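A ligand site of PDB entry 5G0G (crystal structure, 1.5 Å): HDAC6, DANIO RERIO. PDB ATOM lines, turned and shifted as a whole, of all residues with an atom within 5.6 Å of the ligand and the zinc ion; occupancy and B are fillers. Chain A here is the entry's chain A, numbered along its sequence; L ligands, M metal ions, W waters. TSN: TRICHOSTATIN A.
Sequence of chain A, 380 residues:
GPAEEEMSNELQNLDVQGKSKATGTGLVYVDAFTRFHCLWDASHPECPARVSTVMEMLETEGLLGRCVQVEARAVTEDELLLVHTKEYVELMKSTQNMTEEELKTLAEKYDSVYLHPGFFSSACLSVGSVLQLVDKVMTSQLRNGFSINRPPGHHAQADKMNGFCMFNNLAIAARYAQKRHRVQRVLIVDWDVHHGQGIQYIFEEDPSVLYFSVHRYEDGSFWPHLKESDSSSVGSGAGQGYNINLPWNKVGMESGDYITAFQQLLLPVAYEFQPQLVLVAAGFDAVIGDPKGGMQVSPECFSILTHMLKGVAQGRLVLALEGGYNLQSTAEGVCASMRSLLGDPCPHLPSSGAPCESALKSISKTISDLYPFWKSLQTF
A nitrogen (N1) of the ligand is in hydrogen-bond range of a ring nitrogen (NE2) of His 154 (3.3 Å). OH of Tyr 325 lies close to O2 of the ligand. A nitrogen (N1) of the ligand lies within hydrogen-bond range of a ring nitrogen (NE2) of His 155 (2.7 Å). The side-chain amino group (NZ) of Lys 292 lies close to an oxygen (O3) of the ligand, 3.4 Å away.
OD1 of Asp 285 sits at hydrogen-bond distance from N of Val 193, 2.8 Å away. N of Gly 323 sits close to OD2 of Asp 192. A ring nitrogen (NE2) of His 155 sits at hydrogen-bond distance from a ring nitrogen (NE2) of His 154 (3.1 Å). The side-chain carboxylate (OE1) of Glu 322 sits at hydrogen-bond distance from the backbone NH (N) of His 154, at 2.9 Å. The backbone carbonyl oxygen (O) of Ser 112 lies within hydrogen-bond range of the backbone NH (N) of Phe 164 (2.9 Å). O of Ser 112 lies close to N of Gly 163 (3.3 Å).
Trp 40 touches the ligand. Ser 112 touches the ligand (OG to C6, 3.6 Å). CA of Gly 163 touches C15 of the ligand, 3.6 Å away. CE2 of Phe 164 touches C10 of the ligand (3.5 Å). Trp 223 touches the ligand. Gly 323 touches the ligand. Within 4 Å of the ligand: Trp 40, Ser 112, His 154, His 155, Gly 163, Phe 164, Asp 192, His 194, Trp 223, Asp 285, Lys 292, Gly 323 and Tyr 325.
Gly 323 touches the zinc ion. Four residues have an atom within 4 Å of the zinc ion: Asp 192, His 194, Asp 285 and Gly 323. The nearest printed residue that does not touch the zinc ion is His 154 (4.3 Å).
O1 of the ligand binds the zinc ion, at 2.0 Å. OD2 of Asp 285 is bound to the zinc ion (2.0 Å). OD1 of Asp 192 is bound to the zinc ion (2.0 Å). The zinc ion is bound by ND1 of His 194, at 2.2 Å. O2 of the ligand is bound to the zinc ion (2.2 Å). The zinc ion is bound by OD2 of Asp 192, 2.4 Å away. The zinc ion has six donor atoms within binding distance.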
ATOM      1  N   TRP A  40     -29.793  16.219  15.275  1.00  0.00           N
ATOM      2  CA  TRP A  40     -30.242  16.521  16.634  1.00  0.00           C
ATOM      3  C   TRP A  40     -29.178  16.303  17.696  1.00  0.00           C
ATOM      4  O   TRP A  40     -29.469  16.495  18.884  1.00  0.00           O
ATOM      5  CB  TRP A  40     -31.515  15.729  16.972  1.00  0.00           C
ATOM      6  CG  TRP A  40     -31.461  14.284  16.532  1.00  0.00           C
ATOM      7  CD1 TRP A  40     -31.936  13.775  15.357  1.00  0.00           C
ATOM      8  CD2 TRP A  40     -30.888  13.179  17.243  1.00  0.00           C
ATOM      9  NE1 TRP A  40     -31.706  12.425  15.291  1.00  0.00           N
ATOM     10  CE2 TRP A  40     -31.065  12.033  16.434  1.00  0.00           C
ATOM     11  CE3 TRP A  40     -30.253  13.045  18.477  1.00  0.00           C
ATOM     12  CZ2 TRP A  40     -30.624  10.764  16.829  1.00  0.00           C
ATOM     13  CZ3 TRP A  40     -29.807  11.782  18.866  1.00  0.00           C
ATOM     14  CH2 TRP A  40     -29.999  10.663  18.043  1.00  0.00           C
ATOM     15  N   ASP A  41     -27.960  15.906  17.312  1.00  0.00           N
ATOM     16  CA  ASP A  41     -26.886  15.657  18.272  1.00  0.00           C
ATOM     17  C   ASP A  41     -25.563  15.934  17.559  1.00  0.00           C
ATOM     18  O   ASP A  41     -25.085  15.095  16.790  1.00  0.00           O
ATOM     19  CB  ASP A  41     -26.964  14.236  18.782  1.00  0.00           C
ATOM     20  CG  ASP A  41     -26.010  13.963  19.947  1.00  0.00           C
ATOM     21  OD1 ASP A  41     -25.164  14.832  20.247  1.00  0.00           O
ATOM     22  OD2 ASP A  41     -26.111  12.864  20.537  1.00  0.00           O
ATOM     23  N   HIS A  44     -22.953  13.114  17.903  1.00  0.00           N
ATOM     24  CA  HIS A  44     -23.312  11.734  17.615  1.00  0.00           C
ATOM     25  C   HIS A  44     -22.072  10.956  17.203  1.00  0.00           C
ATOM     26  O   HIS A  44     -21.230  11.479  16.457  1.00  0.00           O
ATOM     27  CB  HIS A  44     -24.359  11.676  16.498  1.00  0.00           C
ATOM     28  CG  HIS A  44     -25.036  10.347  16.397  1.00  0.00           C
ATOM     29  ND1 HIS A  44     -24.434   9.248  15.819  1.00  0.00           N
ATOM     30  CD2 HIS A  44     -26.255   9.929  16.810  1.00  0.00           C
ATOM     31  CE1 HIS A  44     -25.258   8.214  15.889  1.00  0.00           C
ATOM     32  NE2 HIS A  44     -26.371   8.596  16.488  1.00  0.00           N
ATOM     33  N   PRO A  45     -21.902   9.717  17.672  1.00  0.00           N
ATOM     34  CA  PRO A  45     -20.655   8.986  17.389  1.00  0.00           C
ATOM     35  C   PRO A  45     -20.457   8.653  15.918  1.00  0.00           C
ATOM     36  O   PRO A  45     -19.307   8.574  15.470  1.00  0.00           O
ATOM     37  CB  PRO A  45     -20.766   7.729  18.254  1.00  0.00           C
ATOM     38  CG  PRO A  45     -22.248   7.566  18.499  1.00  0.00           C
ATOM     39  CD  PRO A  45     -22.778   8.964  18.591  1.00  0.00           C
ATOM     40  N   SER A 112     -31.971   2.536  16.480  1.00  0.00           N
ATOM     41  CA  SER A 112     -30.658   3.187  16.486  1.00  0.00           C
ATOM     42  C   SER A 112     -30.267   3.726  15.112  1.00  0.00           C
ATOM     43  O   SER A 112     -29.266   3.328  14.515  1.00  0.00           O
ATOM     44  CB  SER A 112     -29.588   2.263  17.079  1.00  0.00           C
ATOM     45  OG  SER A 112     -29.893   1.929  18.416  1.00  0.00           O
ATOM     46  N   HIS A 154     -23.681  -3.355   7.755  1.00  0.00           N
ATOM     47  CA  HIS A 154     -23.917  -4.760   8.106  1.00  0.00           C
ATOM     48  C   HIS A 154     -25.210  -5.011   8.898  1.00  0.00           C
ATOM     49  O   HIS A 154     -25.628  -6.172   9.002  1.00  0.00           O
ATOM     50  CB  HIS A 154     -22.698  -5.439   8.747  1.00  0.00           C
ATOM     51  CG  HIS A 154     -22.335  -4.955  10.116  1.00  0.00           C
ATOM     52  ND1 HIS A 154     -21.706  -5.773  11.037  1.00  0.00           N
ATOM     53  CD2 HIS A 154     -22.461  -3.747  10.711  1.00  0.00           C
ATOM     54  CE1 HIS A 154     -21.474  -5.084  12.155  1.00  0.00           C
ATOM     55  NE2 HIS A 154     -21.918  -3.852  11.972  1.00  0.00           N
ATOM     56  N   HIS A 155     -25.864  -3.972   9.412  1.00  0.00           N
ATOM     57  CA  HIS A 155     -27.142  -4.134  10.097  1.00  0.00           C
ATOM     58  C   HIS A 155     -28.342  -3.915   9.192  1.00  0.00           C
ATOM     59  O   HIS A 155     -29.463  -4.262   9.586  1.00  0.00           O
ATOM     60  CB  HIS A 155     -27.265  -3.143  11.263  1.00  0.00           C
ATOM     61  CG  HIS A 155     -26.177  -3.289  12.271  1.00  0.00           C
ATOM     62  ND1 HIS A 155     -25.935  -4.465  12.931  1.00  0.00           N
ATOM     63  CD2 HIS A 155     -25.256  -2.398  12.708  1.00  0.00           C
ATOM     64  CE1 HIS A 155     -24.906  -4.306  13.743  1.00  0.00           C
ATOM     65  NE2 HIS A 155     -24.475  -3.061  13.620  1.00  0.00           N
ATOM     66  N   GLY A 163     -29.296   0.357  13.070  1.00  0.00           N
ATOM     67  CA  GLY A 163     -27.941   0.469  13.578  1.00  0.00           C
ATOM     68  C   GLY A 163     -27.019   1.326  12.731  1.00  0.00           C
ATOM     69  O   GLY A 163     -25.901   0.913  12.419  1.00  0.00           O
ATOM     70  N   PHE A 164     -27.481   2.528  12.365  1.00  0.00           N
ATOM     71  CA  PHE A 164     -26.737   3.491  11.560  1.00  0.00           C
ATOM     72  C   PHE A 164     -26.611   3.112  10.087  1.00  0.00           C
ATOM     73  O   PHE A 164     -25.898   3.813   9.348  1.00  0.00           O
ATOM     74  CB  PHE A 164     -25.333   3.826  12.117  1.00  0.00           C
ATOM     75  CG  PHE A 164     -25.282   4.089  13.600  1.00  0.00           C
ATOM     76  CD1 PHE A 164     -26.355   4.667  14.262  1.00  0.00           C
ATOM     77  CD2 PHE A 164     -24.140   3.779  14.328  1.00  0.00           C
ATOM     78  CE1 PHE A 164     -26.292   4.912  15.625  1.00  0.00           C
ATOM     79  CE2 PHE A 164     -24.061   4.022  15.685  1.00  0.00           C
ATOM     80  CZ  PHE A 164     -25.143   4.586  16.342  1.00  0.00           C
ATOM     81  N   ASP A 192     -16.211  -6.385  13.180  1.00  0.00           N
ATOM     82  CA  ASP A 192     -16.840  -5.337  13.971  1.00  0.00           C
ATOM     83  C   ASP A 192     -17.362  -5.954  15.271  1.00  0.00           C
ATOM     84  O   ASP A 192     -17.756  -7.123  15.305  1.00  0.00           O
ATOM     85  CB  ASP A 192     -17.977  -4.730  13.146  1.00  0.00           C
ATOM     86  CG  ASP A 192     -18.687  -3.593  13.842  1.00  0.00           C
ATOM     87  OD1 ASP A 192     -19.411  -3.837  14.817  1.00  0.00           O
ATOM     88  OD2 ASP A 192     -18.563  -2.448  13.376  1.00  0.00           O
ATOM     89  N   VAL A 193     -17.292  -5.181  16.358  1.00  0.00           N
ATOM     90  CA  VAL A 193     -17.648  -5.684  17.682  1.00  0.00           C
ATOM     91  C   VAL A 193     -19.119  -6.022  17.809  1.00  0.00           C
ATOM     92  O   VAL A 193     -19.519  -6.676  18.782  1.00  0.00           O
ATOM     93  CB  VAL A 193     -17.207  -4.702  18.795  1.00  0.00           C
ATOM     94  CG1 VAL A 193     -18.258  -3.614  18.986  1.00  0.00           C
ATOM     95  CG2 VAL A 193     -16.951  -5.448  20.105  1.00  0.00           C
ATOM     96  N   HIS A 194     -19.939  -5.602  16.850  1.00  0.00           N
ATOM     97  CA  HIS A 194     -21.358  -5.898  16.852  1.00  0.00           C
ATOM     98  C   HIS A 194     -21.661  -7.031  15.874  1.00  0.00           C
ATOM     99  O   HIS A 194     -20.921  -7.291  14.917  1.00  0.00           O
ATOM    100  CB  HIS A 194     -22.162  -4.664  16.466  1.00  0.00           C
ATOM    101  CG  HIS A 194     -21.946  -3.489  17.377  1.00  0.00           C
ATOM    102  ND1 HIS A 194     -21.073  -2.464  17.082  1.00  0.00           N
ATOM    103  CD2 HIS A 194     -22.505  -3.188  18.580  1.00  0.00           C
ATOM    104  CE1 HIS A 194     -21.111  -1.567  18.060  1.00  0.00           C
ATOM    105  NE2 HIS A 194     -21.968  -1.993  18.983  1.00  0.00           N
ATOM    106  N   TRP A 223     -26.090  -4.677  22.612  1.00  0.00           N
ATOM    107  CA  TRP A 223     -26.832  -4.407  21.388  1.00  0.00           C
ATOM    108  C   TRP A 223     -26.272  -5.259  20.225  1.00  0.00           C
ATOM    109  O   TRP A 223     -25.053  -5.398  20.096  1.00  0.00           O
ATOM    110  CB  TRP A 223     -26.749  -2.899  21.062  1.00  0.00           C
ATOM    111  CG  TRP A 223     -27.659  -2.486  19.970  1.00  0.00           C
ATOM    112  CD1 TRP A 223     -28.942  -2.031  20.099  1.00  0.00           C
ATOM    113  CD2 TRP A 223     -27.396  -2.547  18.560  1.00  0.00           C
ATOM    114  NE1 TRP A 223     -29.476  -1.781  18.859  1.00  0.00           N
ATOM    115  CE2 TRP A 223     -28.550  -2.094  17.900  1.00  0.00           C
ATOM    116  CE3 TRP A 223     -26.283  -2.930  17.805  1.00  0.00           C
ATOM    117  CZ2 TRP A 223     -28.635  -2.013  16.513  1.00  0.00           C
ATOM    118  CZ3 TRP A 223     -26.357  -2.855  16.435  1.00  0.00           C
ATOM    119  CH2 TRP A 223     -27.527  -2.399  15.798  1.00  0.00           C
ATOM    120  N   ASP A 285     -14.529  -1.040  16.227  1.00  0.00           N
ATOM    121  CA  ASP A 285     -15.043  -0.801  17.557  1.00  0.00           C
ATOM    122  C   ASP A 285     -14.615  -1.855  18.576  1.00  0.00           C
ATOM    123  O   ASP A 285     -14.949  -1.690  19.756  1.00  0.00           O
ATOM    124  CB  ASP A 285     -16.560  -0.585  17.570  1.00  0.00           C
ATOM    125  CG  ASP A 285     -17.300  -1.421  16.547  1.00  0.00           C
ATOM    126  OD1 ASP A 285     -16.752  -2.449  16.079  1.00  0.00           O
ATOM    127  OD2 ASP A 285     -18.459  -1.049  16.243  1.00  0.00           O
ATOM    128  N   LYS A 292     -17.572   2.375  22.828  1.00  0.00           N
ATOM    129  CA  LYS A 292     -18.742   1.501  22.813  1.00  0.00           C
ATOM    130  C   LYS A 292     -18.389   0.034  22.938  1.00  0.00           C
ATOM    131  O   LYS A 292     -19.129  -0.717  23.578  1.00  0.00           O
ATOM    132  CB  LYS A 292     -19.510   1.672  21.506  1.00  0.00           C
ATOM    133  CG  LYS A 292     -20.056   3.051  21.240  1.00  0.00           C
ATOM    134  CD  LYS A 292     -20.910   2.992  20.006  1.00  0.00           C
ATOM    135  CE  LYS A 292     -21.276   4.371  19.537  1.00  0.00           C
ATOM    136  NZ  LYS A 292     -21.904   4.324  18.192  1.00  0.00           N
ATOM    137  N   GLU A 322     -17.103  -0.531   8.671  1.00  0.00           N
ATOM    138  CA  GLU A 322     -18.371  -0.585   9.375  1.00  0.00           C
ATOM    139  C   GLU A 322     -18.303   0.389  10.548  1.00  0.00           C
ATOM    140  O   GLU A 322     -18.225   1.601  10.319  1.00  0.00           O
ATOM    141  CB  GLU A 322     -18.709  -2.034   9.800  1.00  0.00           C
ATOM    142  CG  GLU A 322     -18.830  -3.012   8.616  1.00  0.00           C
ATOM    143  CD  GLU A 322     -20.152  -2.915   7.850  1.00  0.00           C
ATOM    144  OE1 GLU A 322     -21.052  -2.182   8.300  1.00  0.00           O
ATOM    145  OE2 GLU A 322     -20.301  -3.588   6.806  1.00  0.00           O
ATOM    146  N   GLY A 323     -18.299  -0.116  11.778  1.00  0.00           N
ATOM    147  CA  GLY A 323     -18.246   0.731  12.957  1.00  0.00           C
ATOM    148  C   GLY A 323     -16.829   1.076  13.409  1.00  0.00           C
ATOM    149  O   GLY A 323     -15.843   0.841  12.709  1.00  0.00           O
ATOM    150  N   GLY A 324     -16.751   1.639  14.608  1.00  0.00           N
ATOM    151  CA  GLY A 324     -15.502   2.138  15.156  1.00  0.00           C
ATOM    152  C   GLY A 324     -15.626   3.628  15.418  1.00  0.00           C
ATOM    153  O   GLY A 324     -15.776   4.402  14.476  1.00  0.00           O
ATOM    154  N   TYR A 325     -15.570   4.034  16.685  1.00  0.00           N
ATOM    155  CA  TYR A 325     -15.998   5.369  17.083  1.00  0.00           C
ATOM    156  C   TYR A 325     -14.952   6.195  17.810  1.00  0.00           C
ATOM    157  O   TYR A 325     -15.158   7.397  17.982  1.00  0.00           O
ATOM    158  CB  TYR A 325     -17.290   5.278  17.906  1.00  0.00           C
ATOM    159  CG  TYR A 325     -18.299   4.527  17.092  1.00  0.00           C
ATOM    160  CD1 TYR A 325     -18.951   5.156  16.031  1.00  0.00           C
ATOM    161  CD2 TYR A 325     -18.528   3.172  17.294  1.00  0.00           C
ATOM    162  CE1 TYR A 325     -19.835   4.471  15.245  1.00  0.00           C
ATOM    163  CE2 TYR A 325     -19.429   2.473  16.497  1.00  0.00           C
ATOM    164  CZ  TYR A 325     -20.079   3.133  15.469  1.00  0.00           C
ATOM    165  OH  TYR A 325     -20.966   2.455  14.670  1.00  0.00           O
HETATM  166  O1  TSN L   1     -21.310  -2.186  13.810  1.00  0.00           O
HETATM  167  O2  TSN L   1     -21.083  -0.068  15.386  1.00  0.00           O
HETATM  168  O3  TSN L   1     -24.227   3.450  20.517  1.00  0.00           O
HETATM  169  N1  TSN L   1     -22.387  -1.351  14.094  1.00  0.00           N
HETATM  170  N2  TSN L   1     -28.888   7.755  20.492  1.00  0.00           N
HETATM  171  C1  TSN L   1     -26.287   4.519  20.109  1.00  0.00           C
HETATM  172  C2  TSN L   1     -25.829   5.749  20.538  1.00  0.00           C
HETATM  173  C3  TSN L   1     -26.688   6.826  20.648  1.00  0.00           C
HETATM  174  C4  TSN L   1     -28.036   6.703  20.338  1.00  0.00           C
HETATM  175  C5  TSN L   1     -28.502   5.459  19.904  1.00  0.00           C
HETATM  176  C6  TSN L   1     -27.635   4.381  19.783  1.00  0.00           C
HETATM  177  C7  TSN L   1     -25.355   3.352  20.070  1.00  0.00           C
HETATM  178  C8  TSN L   1     -25.843   2.012  19.512  1.00  0.00           C
HETATM  179  C9  TSN L   1     -24.681   1.554  18.671  1.00  0.00           C
HETATM  180  C10 TSN L   1     -24.777   1.088  17.427  1.00  0.00           C
HETATM  181  C11 TSN L   1     -23.548   0.672  16.767  1.00  0.00           C
HETATM  182  C12 TSN L   1     -23.464   0.001  15.652  1.00  0.00           C
HETATM  183  C13 TSN L   1     -22.206  -0.423  15.005  1.00  0.00           C
HETATM  184  C14 TSN L   1     -26.090   1.039  20.670  1.00  0.00           C
HETATM  185  C15 TSN L   1     -26.067   0.949  16.672  1.00  0.00           C
HETATM  186  C17 TSN L   1     -28.417   9.016  21.023  1.00  0.00           C
HETATM  187  C16 TSN L   1     -30.301   7.621  20.171  1.00  0.00           C
HETATM  188 ZN    ZN M   1     -19.995  -1.931  15.291  1.00  0.00          ZN
HETATM  189  O   HOH W   1     -28.742   7.209  17.243  1.00  0.00           O
HETATM  190  O   HOH W   2     -31.260   7.140  17.012  1.00  0.00           O
